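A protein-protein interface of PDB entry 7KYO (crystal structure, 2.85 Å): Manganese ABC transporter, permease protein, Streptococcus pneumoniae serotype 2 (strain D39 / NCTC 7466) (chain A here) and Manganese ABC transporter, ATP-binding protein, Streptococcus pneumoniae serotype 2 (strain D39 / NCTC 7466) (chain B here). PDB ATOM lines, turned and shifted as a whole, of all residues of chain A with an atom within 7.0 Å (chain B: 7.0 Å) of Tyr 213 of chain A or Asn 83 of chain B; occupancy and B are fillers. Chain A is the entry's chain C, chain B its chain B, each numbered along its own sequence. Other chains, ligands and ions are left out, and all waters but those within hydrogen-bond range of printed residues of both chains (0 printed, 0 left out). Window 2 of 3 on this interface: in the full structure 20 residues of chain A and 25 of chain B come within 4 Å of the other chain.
N of Ile 131 of chain B is in hydrogen-bond range of O of Ile 86 of chain B (3.4 Å). The backbone NH (N) of Asn 83 of chain B sits close to the side-chain carboxylate (OD1) of Asp 81 of chain B (3.3 Å).
CD1 of Leu 38 of chain A touches CE2 of Phe 84 of chain B, 3.5 Å away. Leu 38 of chain A touches Pro 85 of chain B (CD2 to CD, 3.7 Å). CE1 of Phe 162 of chain A touches CG2 of Ile 80 of chain B (3.3 Å). Phe 162 of chain A touches Asp 81 of chain B. CD1 of Phe 162 of chain A touches CG of Phe 84 of chain B, 3.5 Å away. Ile 86 of chain B touches Phe 162 of chain A (CG2 to CE1, 3.9998 Å). Phe 162 of chain A touches Ile 131 of chain B (CE1 to CD1, 3.6 Å). Tyr 213 of chain A touches Pro 85 of chain B (CE1 to CD, 3.9 Å). Ala 216 of chain A touches Pro 85 of chain B.
Tyr 213 of chain A touches just these residues of chain B: Asn 83 (2.7 Å) and Pro 85 (3.9 Å). Printed residues of chain B within 4 Å of Asn 217 of chain A: Gln 130. Of chain A, only Tyr 213 comes within 4 Å of Asn 83 of chain B. Of the printed residues of chain A, Phe 84 of chain B touches Leu 38 and Phe 162. The nearest residue of chain A that does not touch Asn 83 of chain B is Leu 38 of chain A (5.6 Å).
Of the 20 printed residues of chain A, 5 touch a printed residue of chain B. Hydrophobic or aromatic side chains of chain A that line the printed part of chain B: Leu 38, Phe 162 and Tyr 213. Of the 10 printed residues of chain B, 8 touch a printed residue of chain A.
OE1 of Gln 130 of chain B lies close to O of Asn 217 of chain A (3.0 Å). The backbone carbonyl oxygen of Asn 83 of chain B lies within hydrogen-bond range of the side-chain hydroxyl of Tyr 213 of chain A.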
ATOM      1  N   CYS A  34      27.106  27.740  19.493  1.00  0.00           N
ATOM      2  CA  CYS A  34      27.670  26.899  20.562  1.00  0.00           C
ATOM      3  C   CYS A  34      28.278  27.705  21.698  1.00  0.00           C
ATOM      4  O   CYS A  34      28.014  27.433  22.867  1.00  0.00           O
ATOM      5  CB  CYS A  34      28.736  25.957  20.001  1.00  0.00           C
ATOM      6  SG  CYS A  34      28.043  24.549  19.119  1.00  0.00           S
ATOM      7  N   ILE A  37      25.373  29.779  23.842  1.00  0.00           N
ATOM      8  CA  ILE A  37      24.612  29.043  24.871  1.00  0.00           C
ATOM      9  C   ILE A  37      25.464  28.572  26.058  1.00  0.00           C
ATOM     10  O   ILE A  37      24.954  28.473  27.176  1.00  0.00           O
ATOM     11  CB  ILE A  37      23.799  27.848  24.304  1.00  0.00           C
ATOM     12  CG1 ILE A  37      24.694  26.773  23.670  1.00  0.00           C
ATOM     13  CG2 ILE A  37      22.770  28.342  23.299  1.00  0.00           C
ATOM     14  CD1 ILE A  37      24.027  25.416  23.602  1.00  0.00           C
ATOM     15  N   LEU A  38      26.745  28.286  25.813  1.00  0.00           N
ATOM     16  CA  LEU A  38      27.661  27.835  26.870  1.00  0.00           C
ATOM     17  C   LEU A  38      28.070  28.980  27.786  1.00  0.00           C
ATOM     18  O   LEU A  38      28.045  28.835  29.008  1.00  0.00           O
ATOM     19  CB  LEU A  38      28.917  27.188  26.282  1.00  0.00           C
ATOM     20  CG  LEU A  38      28.779  25.842  25.562  1.00  0.00           C
ATOM     21  CD1 LEU A  38      30.113  25.479  24.910  1.00  0.00           C
ATOM     22  CD2 LEU A  38      28.300  24.747  26.506  1.00  0.00           C
ATOM     23  N   PHE A 162      34.921  27.531  29.216  1.00  0.00           N
ATOM     24  CA  PHE A 162      34.745  26.539  30.288  1.00  0.00           C
ATOM     25  C   PHE A 162      35.214  27.042  31.652  1.00  0.00           C
ATOM     26  O   PHE A 162      34.494  26.903  32.640  1.00  0.00           O
ATOM     27  CB  PHE A 162      35.478  25.238  29.931  1.00  0.00           C
ATOM     28  CG  PHE A 162      35.553  24.241  31.060  1.00  0.00           C
ATOM     29  CD1 PHE A 162      34.397  23.741  31.646  1.00  0.00           C
ATOM     30  CD2 PHE A 162      36.786  23.786  31.528  1.00  0.00           C
ATOM     31  CE1 PHE A 162      34.467  22.815  32.679  1.00  0.00           C
ATOM     32  CE2 PHE A 162      36.861  22.861  32.560  1.00  0.00           C
ATOM     33  CZ  PHE A 162      35.700  22.373  33.135  1.00  0.00           C
ATOM     34  N   THR A 207      19.053  27.381  18.809  1.00  0.00           N
ATOM     35  CA  THR A 207      18.300  26.121  18.624  1.00  0.00           C
ATOM     36  C   THR A 207      19.157  24.946  18.103  1.00  0.00           C
ATOM     37  O   THR A 207      19.071  23.845  18.657  1.00  0.00           O
ATOM     38  CB  THR A 207      17.022  26.314  17.759  1.00  0.00           C
ATOM     39  OG1 THR A 207      16.204  27.339  18.335  1.00  0.00           O
ATOM     40  CG2 THR A 207      16.210  25.021  17.669  1.00  0.00           C
ATOM     41  N   PRO A 208      19.979  25.166  17.051  1.00  0.00           N
ATOM     42  CA  PRO A 208      20.911  24.100  16.641  1.00  0.00           C
ATOM     43  C   PRO A 208      21.975  23.768  17.696  1.00  0.00           C
ATOM     44  O   PRO A 208      22.333  22.601  17.858  1.00  0.00           O
ATOM     45  CB  PRO A 208      21.572  24.665  15.375  1.00  0.00           C
ATOM     46  CG  PRO A 208      20.658  25.733  14.895  1.00  0.00           C
ATOM     47  CD  PRO A 208      20.026  26.309  16.122  1.00  0.00           C
ATOM     48  N   ALA A 209      22.471  24.792  18.391  1.00  0.00           N
ATOM     49  CA  ALA A 209      23.454  24.616  19.460  1.00  0.00           C
ATOM     50  C   ALA A 209      22.873  23.868  20.657  1.00  0.00           C
ATOM     51  O   ALA A 209      23.540  23.010  21.230  1.00  0.00           O
ATOM     52  CB  ALA A 209      24.006  25.964  19.896  1.00  0.00           C
ATOM     53  N   ALA A 210      21.636  24.197  21.026  1.00  0.00           N
ATOM     54  CA  ALA A 210      20.928  23.509  22.114  1.00  0.00           C
ATOM     55  C   ALA A 210      20.631  22.048  21.779  1.00  0.00           C
ATOM     56  O   ALA A 210      20.699  21.190  22.659  1.00  0.00           O
ATOM     57  CB  ALA A 210      19.637  24.238  22.455  1.00  0.00           C
ATOM     58  N   THR A 211      20.298  21.778  20.515  1.00  0.00           N
ATOM     59  CA  THR A 211      20.098  20.408  20.029  1.00  0.00           C
ATOM     60  C   THR A 211      21.397  19.605  20.112  1.00  0.00           C
ATOM     61  O   THR A 211      21.411  18.494  20.641  1.00  0.00           O
ATOM     62  CB  THR A 211      19.603  20.382  18.565  1.00  0.00           C
ATOM     63  OG1 THR A 211      18.499  21.280  18.408  1.00  0.00           O
ATOM     64  CG2 THR A 211      19.170  18.972  18.154  1.00  0.00           C
ATOM     65  N   ALA A 212      22.476  20.184  19.589  1.00  0.00           N
ATOM     66  CA  ALA A 212      23.805  19.564  19.627  1.00  0.00           C
ATOM     67  C   ALA A 212      24.315  19.344  21.052  1.00  0.00           C
ATOM     68  O   ALA A 212      25.016  18.365  21.314  1.00  0.00           O
ATOM     69  CB  ALA A 212      24.801  20.408  18.845  1.00  0.00           C
ATOM     70  N   TYR A 213      23.947  20.249  21.960  1.00  0.00           N
ATOM     71  CA  TYR A 213      24.341  20.180  23.374  1.00  0.00           C
ATOM     72  C   TYR A 213      23.756  18.965  24.112  1.00  0.00           C
ATOM     73  O   TYR A 213      24.330  18.506  25.102  1.00  0.00           O
ATOM     74  CB  TYR A 213      23.947  21.492  24.071  1.00  0.00           C
ATOM     75  CG  TYR A 213      24.450  21.723  25.488  1.00  0.00           C
ATOM     76  CD1 TYR A 213      25.694  21.250  25.921  1.00  0.00           C
ATOM     77  CD2 TYR A 213      23.696  22.484  26.381  1.00  0.00           C
ATOM     78  CE1 TYR A 213      26.142  21.493  27.213  1.00  0.00           C
ATOM     79  CE2 TYR A 213      24.138  22.736  27.671  1.00  0.00           C
ATOM     80  CZ  TYR A 213      25.359  22.242  28.086  1.00  0.00           C
ATOM     81  OH  TYR A 213      25.789  22.500  29.371  1.00  0.00           O
ATOM     82  N   LEU A 214      22.631  18.439  23.623  1.00  0.00           N
ATOM     83  CA  LEU A 214      22.042  17.212  24.167  1.00  0.00           C
ATOM     84  C   LEU A 214      22.856  15.961  23.820  1.00  0.00           C
ATOM     85  O   LEU A 214      22.889  15.017  24.611  1.00  0.00           O
ATOM     86  CB  LEU A 214      20.599  17.035  23.681  1.00  0.00           C
ATOM     87  CG  LEU A 214      19.598  18.144  24.034  1.00  0.00           C
ATOM     88  CD1 LEU A 214      18.274  17.876  23.336  1.00  0.00           C
ATOM     89  CD2 LEU A 214      19.411  18.300  25.542  1.00  0.00           C
ATOM     90  N   TYR A 215      23.494  15.954  22.644  1.00  0.00           N
ATOM     91  CA  TYR A 215      24.326  14.824  22.192  1.00  0.00           C
ATOM     92  C   TYR A 215      25.811  14.958  22.531  1.00  0.00           C
ATOM     93  O   TYR A 215      26.471  13.958  22.807  1.00  0.00           O
ATOM     94  CB  TYR A 215      24.216  14.647  20.674  1.00  0.00           C
ATOM     95  CG  TYR A 215      22.831  14.326  20.174  1.00  0.00           C
ATOM     96  CD1 TYR A 215      22.350  13.016  20.181  1.00  0.00           C
ATOM     97  CD2 TYR A 215      22.004  15.329  19.677  1.00  0.00           C
ATOM     98  CE1 TYR A 215      21.077  12.718  19.714  1.00  0.00           C
ATOM     99  CE2 TYR A 215      20.732  15.044  19.207  1.00  0.00           C
ATOM    100  CZ  TYR A 215      20.271  13.740  19.230  1.00  0.00           C
ATOM    101  OH  TYR A 215      19.009  13.457  18.767  1.00  0.00           O
ATOM    102  N   ALA A 216      26.328  16.184  22.494  1.00  0.00           N
ATOM    103  CA  ALA A 216      27.776  16.429  22.502  1.00  0.00           C
ATOM    104  C   ALA A 216      28.500  15.983  23.777  1.00  0.00           C
ATOM    105  O   ALA A 216      27.995  16.179  24.884  1.00  0.00           O
ATOM    106  CB  ALA A 216      28.056  17.903  22.242  1.00  0.00           C
ATOM    107  N   ASN A 217      29.675  15.374  23.589  1.00  0.00           N
ATOM    108  CA  ASN A 217      30.616  15.045  24.669  1.00  0.00           C
ATOM    109  C   ASN A 217      31.942  15.826  24.553  1.00  0.00           C
ATOM    110  O   ASN A 217      32.909  15.526  25.259  1.00  0.00           O
ATOM    111  CB  ASN A 217      30.894  13.533  24.675  1.00  0.00           C
ATOM    112  CG  ASN A 217      29.657  12.705  24.995  1.00  0.00           C
ATOM    113  OD1 ASN A 217      28.857  13.062  25.863  1.00  0.00           O
ATOM    114  ND2 ASN A 217      29.505  11.582  24.300  1.00  0.00           N
ATOM    115  N   MET A 222      30.218  19.300  19.578  1.00  0.00           N
ATOM    116  CA  MET A 222      29.033  20.164  19.589  1.00  0.00           C
ATOM    117  C   MET A 222      28.990  21.103  18.380  1.00  0.00           C
ATOM    118  O   MET A 222      27.912  21.360  17.849  1.00  0.00           O
ATOM    119  CB  MET A 222      28.947  20.977  20.886  1.00  0.00           C
ATOM    120  CG  MET A 222      27.551  21.536  21.150  1.00  0.00           C
ATOM    121  SD  MET A 222      27.319  22.397  22.722  1.00  0.00           S
ATOM    122  CE  MET A 222      28.639  23.593  22.680  1.00  0.00           C
ATOM    123  N   LEU A 225      28.008  19.084  15.118  1.00  0.00           N
ATOM    124  CA  LEU A 225      26.578  18.753  15.201  1.00  0.00           C
ATOM    125  C   LEU A 225      25.698  19.987  14.998  1.00  0.00           C
ATOM    126  O   LEU A 225      24.793  19.973  14.162  1.00  0.00           O
ATOM    127  CB  LEU A 225      26.238  18.071  16.538  1.00  0.00           C
ATOM    128  CG  LEU A 225      26.352  16.541  16.606  1.00  0.00           C
ATOM    129  CD1 LEU A 225      27.579  15.998  15.880  1.00  0.00           C
ATOM    130  CD2 LEU A 225      26.336  16.081  18.059  1.00  0.00           C
ATOM    131  N   SER A 226      25.982  21.048  15.752  1.00  0.00           N
ATOM    132  CA  SER A 226      25.195  22.289  15.701  1.00  0.00           C
ATOM    133  C   SER A 226      25.157  22.908  14.305  1.00  0.00           C
ATOM    134  O   SER A 226      24.105  23.369  13.862  1.00  0.00           O
ATOM    135  CB  SER A 226      25.740  23.315  16.700  1.00  0.00           C
ATOM    136  OG  SER A 226      24.968  24.502  16.686  1.00  0.00           O
ATOM    137  N   PHE A 229      23.016  20.468  12.170  1.00  0.00           N
ATOM    138  CA  PHE A 229      21.605  20.669  12.559  1.00  0.00           C
ATOM    139  C   PHE A 229      21.047  21.994  12.024  1.00  0.00           C
ATOM    140  O   PHE A 229      19.880  22.066  11.640  1.00  0.00           O
ATOM    141  CB  PHE A 229      21.414  20.632  14.086  1.00  0.00           C
ATOM    142  CG  PHE A 229      21.420  19.246  14.682  1.00  0.00           C
ATOM    143  CD1 PHE A 229      20.510  18.283  14.260  1.00  0.00           C
ATOM    144  CD2 PHE A 229      22.308  18.915  15.707  1.00  0.00           C
ATOM    145  CE1 PHE A 229      20.507  17.012  14.819  1.00  0.00           C
ATOM    146  CE2 PHE A 229      22.309  17.645  16.271  1.00  0.00           C
ATOM    147  CZ  PHE A 229      21.406  16.693  15.827  1.00  0.00           C
ATOM    148  N   LYS A 269      21.847  10.451  26.146  1.00  0.00           N
ATOM    149  CA  LYS A 269      22.140  11.059  27.453  1.00  0.00           C
ATOM    150  C   LYS A 269      20.898  11.421  28.303  1.00  0.00           C
ATOM    151  O   LYS A 269      21.050  11.826  29.456  1.00  0.00           O
ATOM    152  CB  LYS A 269      23.061  12.280  27.281  1.00  0.00           C
ATOM    153  CG  LYS A 269      24.461  11.909  26.803  1.00  0.00           C
ATOM    154  CD  LYS A 269      25.328  13.114  26.452  1.00  0.00           C
ATOM    155  CE  LYS A 269      25.686  13.977  27.657  1.00  0.00           C
ATOM    156  NZ  LYS A 269      24.829  15.192  27.776  1.00  0.00           N
ATOM    157  N   ILE B  80      32.797  26.136  38.460  1.00  0.00           N
ATOM    158  CA  ILE B  80      32.997  25.475  37.166  1.00  0.00           C
ATOM    159  C   ILE B  80      31.668  24.835  36.766  1.00  0.00           C
ATOM    160  O   ILE B  80      31.019  24.171  37.583  1.00  0.00           O
ATOM    161  CB  ILE B  80      34.107  24.396  37.234  1.00  0.00           C
ATOM    162  CG1 ILE B  80      35.459  25.038  37.564  1.00  0.00           C
ATOM    163  CG2 ILE B  80      34.202  23.625  35.918  1.00  0.00           C
ATOM    164  CD1 ILE B  80      36.532  24.050  37.973  1.00  0.00           C
ATOM    165  N   ASP B  81      31.268  25.038  35.511  1.00  0.00           N
ATOM    166  CA  ASP B  81      30.056  24.421  34.983  1.00  0.00           C
ATOM    167  C   ASP B  81      30.340  22.944  34.713  1.00  0.00           C
ATOM    168  O   ASP B  81      31.076  22.607  33.786  1.00  0.00           O
ATOM    169  CB  ASP B  81      29.588  25.132  33.707  1.00  0.00           C
ATOM    170  CG  ASP B  81      28.230  24.635  33.205  1.00  0.00           C
ATOM    171  OD1 ASP B  81      27.495  23.957  33.960  1.00  0.00           O
ATOM    172  OD2 ASP B  81      27.893  24.938  32.039  1.00  0.00           O
ATOM    173  N   TYR B  82      29.744  22.084  35.538  1.00  0.00           N
ATOM    174  CA  TYR B  82      29.897  20.624  35.440  1.00  0.00           C
ATOM    175  C   TYR B  82      29.261  20.071  34.159  1.00  0.00           C
ATOM    176  O   TYR B  82      29.706  19.058  33.619  1.00  0.00           O
ATOM    177  CB  TYR B  82      29.254  19.933  36.655  1.00  0.00           C
ATOM    178  CG  TYR B  82      30.007  20.089  37.963  1.00  0.00           C
ATOM    179  CD1 TYR B  82      29.934  21.264  38.705  1.00  0.00           C
ATOM    180  CD2 TYR B  82      30.772  19.048  38.466  1.00  0.00           C
ATOM    181  CE1 TYR B  82      30.617  21.400  39.898  1.00  0.00           C
ATOM    182  CE2 TYR B  82      31.452  19.174  39.661  1.00  0.00           C
ATOM    183  CZ  TYR B  82      31.375  20.352  40.370  1.00  0.00           C
ATOM    184  OH  TYR B  82      32.054  20.478  41.558  1.00  0.00           O
ATOM    185  N   ASN B  83      28.205  20.738  33.681  1.00  0.00           N
ATOM    186  CA  ASN B  83      27.481  20.310  32.473  1.00  0.00           C
ATOM    187  C   ASN B  83      28.088  20.799  31.145  1.00  0.00           C
ATOM    188  O   ASN B  83      27.513  20.546  30.083  1.00  0.00           O
ATOM    189  CB  ASN B  83      26.006  20.732  32.563  1.00  0.00           C
ATOM    190  CG  ASN B  83      25.281  20.072  33.722  1.00  0.00           C
ATOM    191  OD1 ASN B  83      25.424  18.870  33.961  1.00  0.00           O
ATOM    192  ND2 ASN B  83      24.487  20.855  34.446  1.00  0.00           N
ATOM    193  N   PHE B  84      29.231  21.488  31.196  1.00  0.00           N
ATOM    194  CA  PHE B  84      29.998  21.824  29.986  1.00  0.00           C
ATOM    195  C   PHE B  84      30.457  20.523  29.313  1.00  0.00           C
ATOM    196  O   PHE B  84      30.895  19.606  30.010  1.00  0.00           O
ATOM    197  CB  PHE B  84      31.214  22.695  30.350  1.00  0.00           C
ATOM    198  CG  PHE B  84      31.921  23.296  29.161  1.00  0.00           C
ATOM    199  CD1 PHE B  84      32.905  22.582  28.479  1.00  0.00           C
ATOM    200  CD2 PHE B  84      31.614  24.584  28.728  1.00  0.00           C
ATOM    201  CE1 PHE B  84      33.554  23.132  27.381  1.00  0.00           C
ATOM    202  CE2 PHE B  84      32.263  25.140  27.632  1.00  0.00           C
ATOM    203  CZ  PHE B  84      33.234  24.413  26.959  1.00  0.00           C
ATOM    204  N   PRO B  85      30.353  20.429  27.967  1.00  0.00           N
ATOM    205  CA  PRO B  85      30.714  19.167  27.316  1.00  0.00           C
ATOM    206  C   PRO B  85      32.230  19.007  27.220  1.00  0.00           C
ATOM    207  O   PRO B  85      32.858  19.548  26.307  1.00  0.00           O
ATOM    208  CB  PRO B  85      30.067  19.288  25.936  1.00  0.00           C
ATOM    209  CG  PRO B  85      30.063  20.747  25.653  1.00  0.00           C
ATOM    210  CD  PRO B  85      30.005  21.466  26.975  1.00  0.00           C
ATOM    211  N   ILE B  86      32.801  18.288  28.183  1.00  0.00           N
ATOM    212  CA  ILE B  86      34.250  18.086  28.261  1.00  0.00           C
ATOM    213  C   ILE B  86      34.581  16.815  29.050  1.00  0.00           C
ATOM    214  O   ILE B  86      33.969  16.537  30.084  1.00  0.00           O
ATOM    215  CB  ILE B  86      34.965  19.327  28.862  1.00  0.00           C
ATOM    216  CG1 ILE B  86      36.487  19.175  28.794  1.00  0.00           C
ATOM    217  CG2 ILE B  86      34.519  19.603  30.296  1.00  0.00           C
ATOM    218  CD1 ILE B  86      37.234  20.478  28.984  1.00  0.00           C
ATOM    219  N   GLN B 130      32.524  12.033  31.138  1.00  0.00           N
ATOM    220  CA  GLN B 130      32.205  13.452  31.279  1.00  0.00           C
ATOM    221  C   GLN B 130      32.453  13.863  32.722  1.00  0.00           C
ATOM    222  O   GLN B 130      32.301  13.050  33.638  1.00  0.00           O
ATOM    223  CB  GLN B 130      30.744  13.732  30.918  1.00  0.00           C
ATOM    224  CG  GLN B 130      30.414  13.514  29.451  1.00  0.00           C
ATOM    225  CD  GLN B 130      30.958  14.615  28.565  1.00  0.00           C
ATOM    226  OE1 GLN B 130      32.006  14.462  27.939  1.00  0.00           O
ATOM    227  NE2 GLN B 130      30.254  15.739  28.522  1.00  0.00           N
ATOM    228  N   ILE B 131      32.835  15.121  32.920  1.00  0.00           N
ATOM    229  CA  ILE B 131      33.054  15.657  34.272  1.00  0.00           C
ATOM    230  C   ILE B 131      31.766  15.695  35.122  1.00  0.00           C
ATOM    231  O   ILE B 131      31.836  15.587  36.347  1.00  0.00           O
ATOM    232  CB  ILE B 131      33.768  17.035  34.258  1.00  0.00           C
ATOM    233  CG1 ILE B 131      32.960  18.099  33.504  1.00  0.00           C
ATOM    234  CG2 ILE B 131      35.159  16.899  33.651  1.00  0.00           C
ATOM    235  CD1 ILE B 131      33.489  19.505  33.685  1.00  0.00           C
ATOM    236  N   SER B 132      30.607  15.826  34.471  1.00  0.00           N
ATOM    237  CA  SER B 132      29.304  15.737  35.151  1.00  0.00           C
ATOM    238  C   SER B 132      29.036  14.366  35.780  1.00  0.00           C
ATOM    239  O   SER B 132      28.332  14.272  36.785  1.00  0.00           O
ATOM    240  CB  SER B 132      28.169  16.067  34.178  1.00  0.00           C
ATOM    241  OG  SER B 132      28.241  15.252  33.023  1.00  0.00           O
